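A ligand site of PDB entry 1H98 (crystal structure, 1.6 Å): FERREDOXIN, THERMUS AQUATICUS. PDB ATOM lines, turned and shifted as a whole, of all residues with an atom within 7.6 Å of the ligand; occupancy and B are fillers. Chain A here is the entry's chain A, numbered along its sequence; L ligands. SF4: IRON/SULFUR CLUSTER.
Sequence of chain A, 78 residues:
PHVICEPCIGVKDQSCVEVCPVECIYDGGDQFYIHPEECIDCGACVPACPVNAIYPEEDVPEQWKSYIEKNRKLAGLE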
ATOM      1  N   PRO A   1     -26.019 -26.170 -28.752  1.00  0.00           N
ATOM      2  CA  PRO A   1     -25.006 -27.030 -28.103  1.00  0.00           C
ATOM      3  C   PRO A   1     -24.313 -27.978 -29.099  1.00  0.00           C
ATOM      4  O   PRO A   1     -24.743 -28.057 -30.248  1.00  0.00           O
ATOM      5  CB  PRO A   1     -25.724 -27.834 -27.017  1.00  0.00           C
ATOM      6  CG  PRO A   1     -27.195 -27.599 -27.369  1.00  0.00           C
ATOM      7  CD  PRO A   1     -27.261 -26.211 -27.964  1.00  0.00           C
ATOM      8  N   HIS A   2     -23.177 -28.554 -28.697  1.00  0.00           N
ATOM      9  CA  HIS A   2     -22.456 -29.513 -29.527  1.00  0.00           C
ATOM     10  C   HIS A   2     -22.854 -30.886 -28.978  1.00  0.00           C
ATOM     11  O   HIS A   2     -23.288 -30.994 -27.829  1.00  0.00           O
ATOM     12  CB  HIS A   2     -20.947 -29.303 -29.457  1.00  0.00           C
ATOM     13  CG  HIS A   2     -20.445 -28.260 -30.412  1.00  0.00           C
ATOM     14  ND1 HIS A   2     -20.991 -26.992 -30.480  1.00  0.00           N
ATOM     15  CD2 HIS A   2     -19.456 -28.297 -31.334  1.00  0.00           C
ATOM     16  CE1 HIS A   2     -20.352 -26.296 -31.406  1.00  0.00           C
ATOM     17  NE2 HIS A   2     -19.424 -27.060 -31.936  1.00  0.00           N
ATOM     18  N   VAL A   3     -22.732 -31.929 -29.801  1.00  0.00           N
ATOM     19  CA  VAL A   3     -23.154 -33.262 -29.410  1.00  0.00           C
ATOM     20  C   VAL A   3     -22.087 -34.321 -29.733  1.00  0.00           C
ATOM     21  O   VAL A   3     -21.504 -34.291 -30.802  1.00  0.00           O
ATOM     22  CB  VAL A   3     -24.476 -33.640 -30.165  1.00  0.00           C
ATOM     23  CG1 VAL A   3     -24.943 -35.036 -29.785  1.00  0.00           C
ATOM     24  CG2 VAL A   3     -25.568 -32.601 -29.870  1.00  0.00           C
ATOM     25  N   ILE A   4     -21.832 -35.219 -28.789  1.00  0.00           N
ATOM     26  CA  ILE A   4     -20.864 -36.300 -29.015  1.00  0.00           C
ATOM     27  C   ILE A   4     -21.651 -37.470 -29.591  1.00  0.00           C
ATOM     28  O   ILE A   4     -22.599 -37.983 -28.972  1.00  0.00           O
ATOM     29  CB  ILE A   4     -20.122 -36.728 -27.713  1.00  0.00           C
ATOM     30  CG1 ILE A   4     -19.228 -35.583 -27.218  1.00  0.00           C
ATOM     31  CG2 ILE A   4     -19.311 -37.988 -27.962  1.00  0.00           C
ATOM     32  CD1 ILE A   4     -18.468 -35.877 -25.951  1.00  0.00           C
ATOM     33  N   CYS A  16     -10.954 -34.086 -26.088  1.00  0.00           N
ATOM     34  CA  CYS A  16     -11.964 -33.030 -26.076  1.00  0.00           C
ATOM     35  C   CYS A  16     -12.090 -32.379 -24.705  1.00  0.00           C
ATOM     36  O   CYS A  16     -12.351 -31.176 -24.601  1.00  0.00           O
ATOM     37  CB  CYS A  16     -13.320 -33.592 -26.508  1.00  0.00           C
ATOM     38  SG  CYS A  16     -13.971 -34.940 -25.472  1.00  0.00           S
ATOM     39  N   VAL A  17     -11.901 -33.180 -23.659  1.00  0.00           N
ATOM     40  CA  VAL A  17     -12.029 -32.697 -22.286  1.00  0.00           C
ATOM     41  C   VAL A  17     -11.021 -31.598 -21.952  1.00  0.00           C
ATOM     42  O   VAL A  17     -11.388 -30.592 -21.330  1.00  0.00           O
ATOM     43  CB  VAL A  17     -11.873 -33.859 -21.249  1.00  0.00           C
ATOM     44  CG1 VAL A  17     -11.932 -33.307 -19.827  1.00  0.00           C
ATOM     45  CG2 VAL A  17     -12.984 -34.881 -21.435  1.00  0.00           C
ATOM     46  N   VAL A  19      -9.662 -29.335 -23.871  1.00  0.00           N
ATOM     47  CA  VAL A  19      -9.776 -28.080 -24.600  1.00  0.00           C
ATOM     48  C   VAL A  19     -11.073 -27.314 -24.304  1.00  0.00           C
ATOM     49  O   VAL A  19     -11.206 -26.158 -24.686  1.00  0.00           O
ATOM     50  CB  VAL A  19      -9.611 -28.271 -26.124  1.00  0.00           C
ATOM     51  CG1 VAL A  19      -8.253 -28.908 -26.427  1.00  0.00           C
ATOM     52  CG2 VAL A  19     -10.732 -29.137 -26.691  1.00  0.00           C
ATOM     53  N   CYS A  20     -12.022 -27.952 -23.618  1.00  0.00           N
ATOM     54  CA  CYS A  20     -13.292 -27.300 -23.311  1.00  0.00           C
ATOM     55  C   CYS A  20     -13.128 -26.248 -22.206  1.00  0.00           C
ATOM     56  O   CYS A  20     -12.864 -26.576 -21.051  1.00  0.00           O
ATOM     57  CB  CYS A  20     -14.343 -28.341 -22.920  1.00  0.00           C
ATOM     58  SG  CYS A  20     -15.949 -27.622 -22.511  1.00  0.00           S
ATOM     59  N   PRO A  21     -13.368 -24.963 -22.536  1.00  0.00           N
ATOM     60  CA  PRO A  21     -13.225 -23.866 -21.573  1.00  0.00           C
ATOM     61  C   PRO A  21     -14.168 -23.900 -20.363  1.00  0.00           C
ATOM     62  O   PRO A  21     -13.861 -23.316 -19.323  1.00  0.00           O
ATOM     63  CB  PRO A  21     -13.492 -22.630 -22.439  1.00  0.00           C
ATOM     64  CG  PRO A  21     -14.471 -23.125 -23.450  1.00  0.00           C
ATOM     65  CD  PRO A  21     -13.850 -24.461 -23.838  1.00  0.00           C
ATOM     66  N   VAL A  22     -15.329 -24.542 -20.518  1.00  0.00           N
ATOM     67  CA  VAL A  22     -16.295 -24.603 -19.419  1.00  0.00           C
ATOM     68  C   VAL A  22     -16.386 -25.965 -18.750  1.00  0.00           C
ATOM     69  O   VAL A  22     -17.201 -26.152 -17.844  1.00  0.00           O
ATOM     70  CB  VAL A  22     -17.710 -24.157 -19.872  1.00  0.00           C
ATOM     71  CG1 VAL A  22     -17.686 -22.670 -20.209  1.00  0.00           C
ATOM     72  CG2 VAL A  22     -18.173 -24.962 -21.080  1.00  0.00           C
ATOM     73  N   GLU A  23     -15.544 -26.914 -19.180  1.00  0.00           N
ATOM     74  CA  GLU A  23     -15.510 -28.263 -18.625  1.00  0.00           C
ATOM     75  C   GLU A  23     -16.896 -28.909 -18.537  1.00  0.00           C
ATOM     76  O   GLU A  23     -17.283 -29.440 -17.483  1.00  0.00           O
ATOM     77  CB  GLU A  23     -14.855 -28.248 -17.238  1.00  0.00           C
ATOM     78  CG  GLU A  23     -13.449 -27.653 -17.201  1.00  0.00           C
ATOM     79  CD  GLU A  23     -12.931 -27.402 -15.788  1.00  0.00           C
ATOM     80  OE1 GLU A  23     -13.727 -27.483 -14.821  1.00  0.00           O
ATOM     81  OE2 GLU A  23     -11.722 -27.115 -15.635  1.00  0.00           O
ATOM     82  N   CYS A  24     -17.628 -28.908 -19.647  1.00  0.00           N
ATOM     83  CA  CYS A  24     -18.954 -29.498 -19.675  1.00  0.00           C
ATOM     84  C   CYS A  24     -19.030 -30.838 -20.422  1.00  0.00           C
ATOM     85  O   CYS A  24     -20.091 -31.238 -20.882  1.00  0.00           O
ATOM     86  CB  CYS A  24     -19.946 -28.505 -20.286  1.00  0.00           C
ATOM     87  SG  CYS A  24     -19.616 -28.097 -22.003  1.00  0.00           S
ATOM     88  N   ILE A  25     -17.899 -31.526 -20.533  1.00  0.00           N
ATOM     89  CA  ILE A  25     -17.843 -32.829 -21.189  1.00  0.00           C
ATOM     90  C   ILE A  25     -17.619 -33.844 -20.080  1.00  0.00           C
ATOM     91  O   ILE A  25     -16.610 -33.784 -19.366  1.00  0.00           O
ATOM     92  CB  ILE A  25     -16.723 -32.902 -22.239  1.00  0.00           C
ATOM     93  CG1 ILE A  25     -16.948 -31.850 -23.330  1.00  0.00           C
ATOM     94  CG2 ILE A  25     -16.681 -34.307 -22.866  1.00  0.00           C
ATOM     95  CD1 ILE A  25     -15.873 -31.786 -24.391  1.00  0.00           C
ATOM     96  N   TYR A  33     -20.165 -37.295 -22.913  1.00  0.00           N
ATOM     97  CA  TYR A  33     -21.287 -36.536 -23.444  1.00  0.00           C
ATOM     98  C   TYR A  33     -21.084 -35.076 -23.105  1.00  0.00           C
ATOM     99  O   TYR A  33     -20.312 -34.737 -22.205  1.00  0.00           O
ATOM    100  CB  TYR A  33     -22.610 -37.051 -22.868  1.00  0.00           C
ATOM    101  CG  TYR A  33     -22.786 -36.781 -21.388  1.00  0.00           C
ATOM    102  CD1 TYR A  33     -23.410 -35.620 -20.941  1.00  0.00           C
ATOM    103  CD2 TYR A  33     -22.311 -37.694 -20.442  1.00  0.00           C
ATOM    104  CE1 TYR A  33     -23.558 -35.360 -19.589  1.00  0.00           C
ATOM    105  CE2 TYR A  33     -22.459 -37.438 -19.076  1.00  0.00           C
ATOM    106  CZ  TYR A  33     -23.077 -36.278 -18.667  1.00  0.00           C
ATOM    107  OH  TYR A  33     -23.220 -36.030 -17.311  1.00  0.00           O
ATOM    108  N   ILE A  34     -21.759 -34.219 -23.860  1.00  0.00           N
ATOM    109  CA  ILE A  34     -21.695 -32.780 -23.658  1.00  0.00           C
ATOM    110  C   ILE A  34     -22.981 -32.307 -22.984  1.00  0.00           C
ATOM    111  O   ILE A  34     -24.079 -32.614 -23.453  1.00  0.00           O
ATOM    112  CB  ILE A  34     -21.500 -32.045 -25.013  1.00  0.00           C
ATOM    113  CG1 ILE A  34     -20.087 -32.286 -25.546  1.00  0.00           C
ATOM    114  CG2 ILE A  34     -21.757 -30.544 -24.851  1.00  0.00           C
ATOM    115  CD1 ILE A  34     -19.855 -31.811 -26.970  1.00  0.00           C
ATOM    116  N   HIS A  35     -22.847 -31.614 -21.859  1.00  0.00           N
ATOM    117  CA  HIS A  35     -24.021 -31.110 -21.169  1.00  0.00           C
ATOM    118  C   HIS A  35     -24.558 -29.930 -21.984  1.00  0.00           C
ATOM    119  O   HIS A  35     -23.933 -28.874 -22.045  1.00  0.00           O
ATOM    120  CB  HIS A  35     -23.691 -30.684 -19.748  1.00  0.00           C
ATOM    121  CG  HIS A  35     -24.898 -30.452 -18.901  1.00  0.00           C
ATOM    122  ND1 HIS A  35     -25.141 -31.163 -17.746  1.00  0.00           N
ATOM    123  CD2 HIS A  35     -25.948 -29.615 -19.056  1.00  0.00           C
ATOM    124  CE1 HIS A  35     -26.297 -30.772 -17.221  1.00  0.00           C
ATOM    125  NE2 HIS A  35     -26.802 -29.830 -17.996  1.00  0.00           N
ATOM    126  N   GLU A  38     -24.797 -26.376 -20.416  1.00  0.00           N
ATOM    127  CA  GLU A  38     -23.529 -25.764 -20.035  1.00  0.00           C
ATOM    128  C   GLU A  38     -22.675 -25.359 -21.238  1.00  0.00           C
ATOM    129  O   GLU A  38     -21.920 -24.384 -21.168  1.00  0.00           O
ATOM    130  CB  GLU A  38     -22.723 -26.701 -19.119  1.00  0.00           C
ATOM    131  CG  GLU A  38     -23.407 -27.007 -17.806  1.00  0.00           C
ATOM    132  CD  GLU A  38     -22.614 -27.974 -16.921  1.00  0.00           C
ATOM    133  OE1 GLU A  38     -21.567 -28.500 -17.360  1.00  0.00           O
ATOM    134  OE2 GLU A  38     -23.044 -28.200 -15.770  1.00  0.00           O
ATOM    135  N   CYS A  39     -22.776 -26.135 -22.313  1.00  0.00           N
ATOM    136  CA  CYS A  39     -22.014 -25.870 -23.528  1.00  0.00           C
ATOM    137  C   CYS A  39     -22.255 -24.467 -24.080  1.00  0.00           C
ATOM    138  O   CYS A  39     -23.401 -24.038 -24.230  1.00  0.00           O
ATOM    139  CB  CYS A  39     -22.356 -26.930 -24.582  1.00  0.00           C
ATOM    140  SG  CYS A  39     -21.544 -26.689 -26.173  1.00  0.00           S
ATOM    141  N   ILE A  40     -21.177 -23.749 -24.389  1.00  0.00           N
ATOM    142  CA  ILE A  40     -21.274 -22.393 -24.934  1.00  0.00           C
ATOM    143  C   ILE A  40     -21.088 -22.348 -26.447  1.00  0.00           C
ATOM    144  O   ILE A  40     -20.999 -21.260 -27.042  1.00  0.00           O
ATOM    145  CB  ILE A  40     -20.255 -21.423 -24.270  1.00  0.00           C
ATOM    146  CG1 ILE A  40     -18.827 -21.900 -24.511  1.00  0.00           C
ATOM    147  CG2 ILE A  40     -20.551 -21.288 -22.770  1.00  0.00           C
ATOM    148  CD1 ILE A  40     -17.781 -20.957 -23.950  1.00  0.00           C
ATOM    149  N   ASP A  41     -20.990 -23.520 -27.072  1.00  0.00           N
ATOM    150  CA  ASP A  41     -20.840 -23.638 -28.515  1.00  0.00           C
ATOM    151  C   ASP A  41     -19.620 -22.947 -29.098  1.00  0.00           C
ATOM    152  O   ASP A  41     -19.680 -22.411 -30.208  1.00  0.00           O
ATOM    153  CB  ASP A  41     -22.101 -23.130 -29.230  1.00  0.00           C
ATOM    154  CG  ASP A  41     -23.243 -24.109 -29.145  1.00  0.00           C
ATOM    155  OD1 ASP A  41     -23.054 -25.265 -29.552  1.00  0.00           O
ATOM    156  OD2 ASP A  41     -24.332 -23.735 -28.670  1.00  0.00           O
ATOM    157  N   CYS A  42     -18.491 -22.988 -28.392  1.00  0.00           N
ATOM    158  CA  CYS A  42     -17.286 -22.365 -28.914  1.00  0.00           C
ATOM    159  C   CYS A  42     -16.646 -23.196 -30.030  1.00  0.00           C
ATOM    160  O   CYS A  42     -15.849 -22.684 -30.811  1.00  0.00           O
ATOM    161  CB  CYS A  42     -16.288 -22.122 -27.777  1.00  0.00           C
ATOM    162  SG  CYS A  42     -15.585 -23.628 -27.124  1.00  0.00           S
ATOM    163  N   GLY A  43     -16.968 -24.484 -30.098  1.00  0.00           N
ATOM    164  CA  GLY A  43     -16.452 -25.357 -31.145  1.00  0.00           C
ATOM    165  C   GLY A  43     -15.037 -25.902 -31.001  1.00  0.00           C
ATOM    166  O   GLY A  43     -14.609 -26.713 -31.815  1.00  0.00           O
ATOM    167  N   ALA A  44     -14.336 -25.515 -29.939  1.00  0.00           N
ATOM    168  CA  ALA A  44     -12.960 -25.963 -29.707  1.00  0.00           C
ATOM    169  C   ALA A  44     -12.780 -27.478 -29.637  1.00  0.00           C
ATOM    170  O   ALA A  44     -11.738 -28.007 -30.025  1.00  0.00           O
ATOM    171  CB  ALA A  44     -12.396 -25.305 -28.448  1.00  0.00           C
ATOM    172  N   CYS A  45     -13.797 -28.173 -29.152  1.00  0.00           N
ATOM    173  CA  CYS A  45     -13.745 -29.618 -29.002  1.00  0.00           C
ATOM    174  C   CYS A  45     -13.779 -30.400 -30.308  1.00  0.00           C
ATOM    175  O   CYS A  45     -13.314 -31.546 -30.359  1.00  0.00           O
ATOM    176  CB  CYS A  45     -14.894 -30.074 -28.107  1.00  0.00           C
ATOM    177  SG  CYS A  45     -16.490 -29.544 -28.712  1.00  0.00           S
ATOM    178  N   VAL A  46     -14.312 -29.793 -31.366  1.00  0.00           N
ATOM    179  CA  VAL A  46     -14.423 -30.470 -32.662  1.00  0.00           C
ATOM    180  C   VAL A  46     -13.107 -30.959 -33.268  1.00  0.00           C
ATOM    181  O   VAL A  46     -12.966 -32.141 -33.557  1.00  0.00           O
ATOM    182  CB  VAL A  46     -15.219 -29.622 -33.678  1.00  0.00           C
ATOM    183  CG1 VAL A  46     -15.241 -30.305 -35.043  1.00  0.00           C
ATOM    184  CG2 VAL A  46     -16.645 -29.417 -33.162  1.00  0.00           C
ATOM    185  N   ILE A  54     -17.595 -35.354 -32.604  1.00  0.00           N
ATOM    186  CA  ILE A  54     -18.322 -34.157 -32.183  1.00  0.00           C
ATOM    187  C   ILE A  54     -18.852 -33.266 -33.312  1.00  0.00           C
ATOM    188  O   ILE A  54     -18.101 -32.881 -34.212  1.00  0.00           O
ATOM    189  CB  ILE A  54     -17.467 -33.323 -31.219  1.00  0.00           C
ATOM    190  CG1 ILE A  54     -16.931 -34.223 -30.100  1.00  0.00           C
ATOM    191  CG2 ILE A  54     -18.281 -32.199 -30.613  1.00  0.00           C
ATOM    192  CD1 ILE A  54     -15.985 -33.550 -29.139  1.00  0.00           C
ATOM    193  N   TYR A  55     -20.136 -32.929 -33.215  1.00  0.00           N
ATOM    194  CA  TYR A  55     -20.818 -32.096 -34.206  1.00  0.00           C
ATOM    195  C   TYR A  55     -21.706 -31.043 -33.569  1.00  0.00           C
ATOM    196  O   TYR A  55     -22.213 -31.244 -32.462  1.00  0.00           O
ATOM    197  CB  TYR A  55     -21.778 -32.949 -35.050  1.00  0.00           C
ATOM    198  CG  TYR A  55     -21.128 -33.842 -36.067  1.00  0.00           C
ATOM    199  CD1 TYR A  55     -20.730 -35.134 -35.726  1.00  0.00           C
ATOM    200  CD2 TYR A  55     -20.908 -33.391 -37.365  1.00  0.00           C
ATOM    201  CE1 TYR A  55     -20.123 -35.959 -36.663  1.00  0.00           C
ATOM    202  CE2 TYR A  55     -20.307 -34.203 -38.306  1.00  0.00           C
ATOM    203  CZ  TYR A  55     -19.907 -35.490 -37.949  1.00  0.00           C
ATOM    204  OH  TYR A  55     -19.266 -36.277 -38.890  1.00  0.00           O
ATOM    205  N   PRO A  56     -21.834 -29.864 -34.210  1.00  0.00           N
ATOM    206  CA  PRO A  56     -22.707 -28.834 -33.646  1.00  0.00           C
ATOM    207  C   PRO A  56     -24.079 -29.496 -33.798  1.00  0.00           C
ATOM    208  O   PRO A  56     -24.278 -30.248 -34.755  1.00  0.00           O
ATOM    209  CB  PRO A  56     -22.563 -27.680 -34.641  1.00  0.00           C
ATOM    210  CG  PRO A  56     -21.153 -27.823 -35.109  1.00  0.00           C
ATOM    211  CD  PRO A  56     -21.004 -29.318 -35.305  1.00  0.00           C
HETATM  212 FE1  SF4 L   1     -19.302 -26.845 -25.940  1.00  0.00          FE
HETATM  213 FE2  SF4 L   1     -16.929 -27.258 -24.545  1.00  0.00          FE
HETATM  214 FE3  SF4 L   1     -17.167 -28.130 -27.159  1.00  0.00          FE
HETATM  215 FE4  SF4 L   1     -16.984 -25.435 -26.559  1.00  0.00          FE
HETATM  216  S1  SF4 L   1     -15.345 -27.045 -26.213  1.00  0.00           S
HETATM  217  S2  SF4 L   1     -18.490 -26.477 -28.076  1.00  0.00           S
HETATM  218  S3  SF4 L   1     -18.183 -25.307 -24.608  1.00  0.00           S
HETATM  219  S4  SF4 L   1     -18.395 -28.894 -25.315  1.00  0.00           S
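S1 of the ligand lies close to N of Cys 45 (3.5 Å). The side-chain sulfur (SG) of Cys 45 binds an iron atom (FE3) of the ligand (2.2 Å). The side-chain sulfur of Cys 39 is bound to an iron atom (FE1) of the ligand (2.3 Å). FE2 of the ligand is bound by SG of Cys 20 (2.3 Å). The backbone NH of Cys 42 sits close to a sulfur (S2) of the ligand (3.5 Å). SG of Cys 42 is bound to FE4 of the ligand, 2.4 Å away. S2 of the ligand lies close to N of Gly 43, at 3.2 Å. A sulfur (S3) of the ligand sits close to the backbone NH (N) of Ile 40 (3.4 Å). S2 of the ligand lies close to ND1 of His 2 (3.5 Å). A sulfur (S4) of the ligand lies close to the side-chain sulfur (SG) of Cys 24, 3.6 Å away.
N of His 2 lies close to SG of Cys 39 (3.5 Å). SG of Cys 24 lies close to N of Cys 39. The side-chain sulfur (SG) of Cys 39 sits close to the backbone NH (N) of Asp 41, at 3.3 Å. The backbone NH of Val 22 lies close to the side-chain sulfur of Cys 20 (3.7 Å). The side-chain sulfur (SG) of Cys 20 sits close to the backbone NH (N) of Glu 23 (3.4 Å). SG of Cys 42 lies close to N of Ala 44 (3.6 Å). OD1 of Asp 41 lies within hydrogen-bond range of ND1 of His 2 (2.8 Å). O of Cys 24 sits at hydrogen-bond distance from N of His 35, at 2.9 Å.
Pro 21 touches the ligand (CD to S1, 3.8 Å). CG2 of Val 22 touches S3 of the ligand, at 3.5 Å. Ile 25 touches the ligand. CD1 of Ile 34 touches S4 of the ligand, at 3.7 Å. CA of Asp 41 touches S2 of the ligand, 3.7 Å away. Hydrophobic or aromatic side chains within 4 Å of the ligand: His 2, Pro 21, Val 22, Ile 25, Ile 34 and Ile 40. The nearest printed residue that does not touch the ligand is Ala 44 (4.1 Å).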
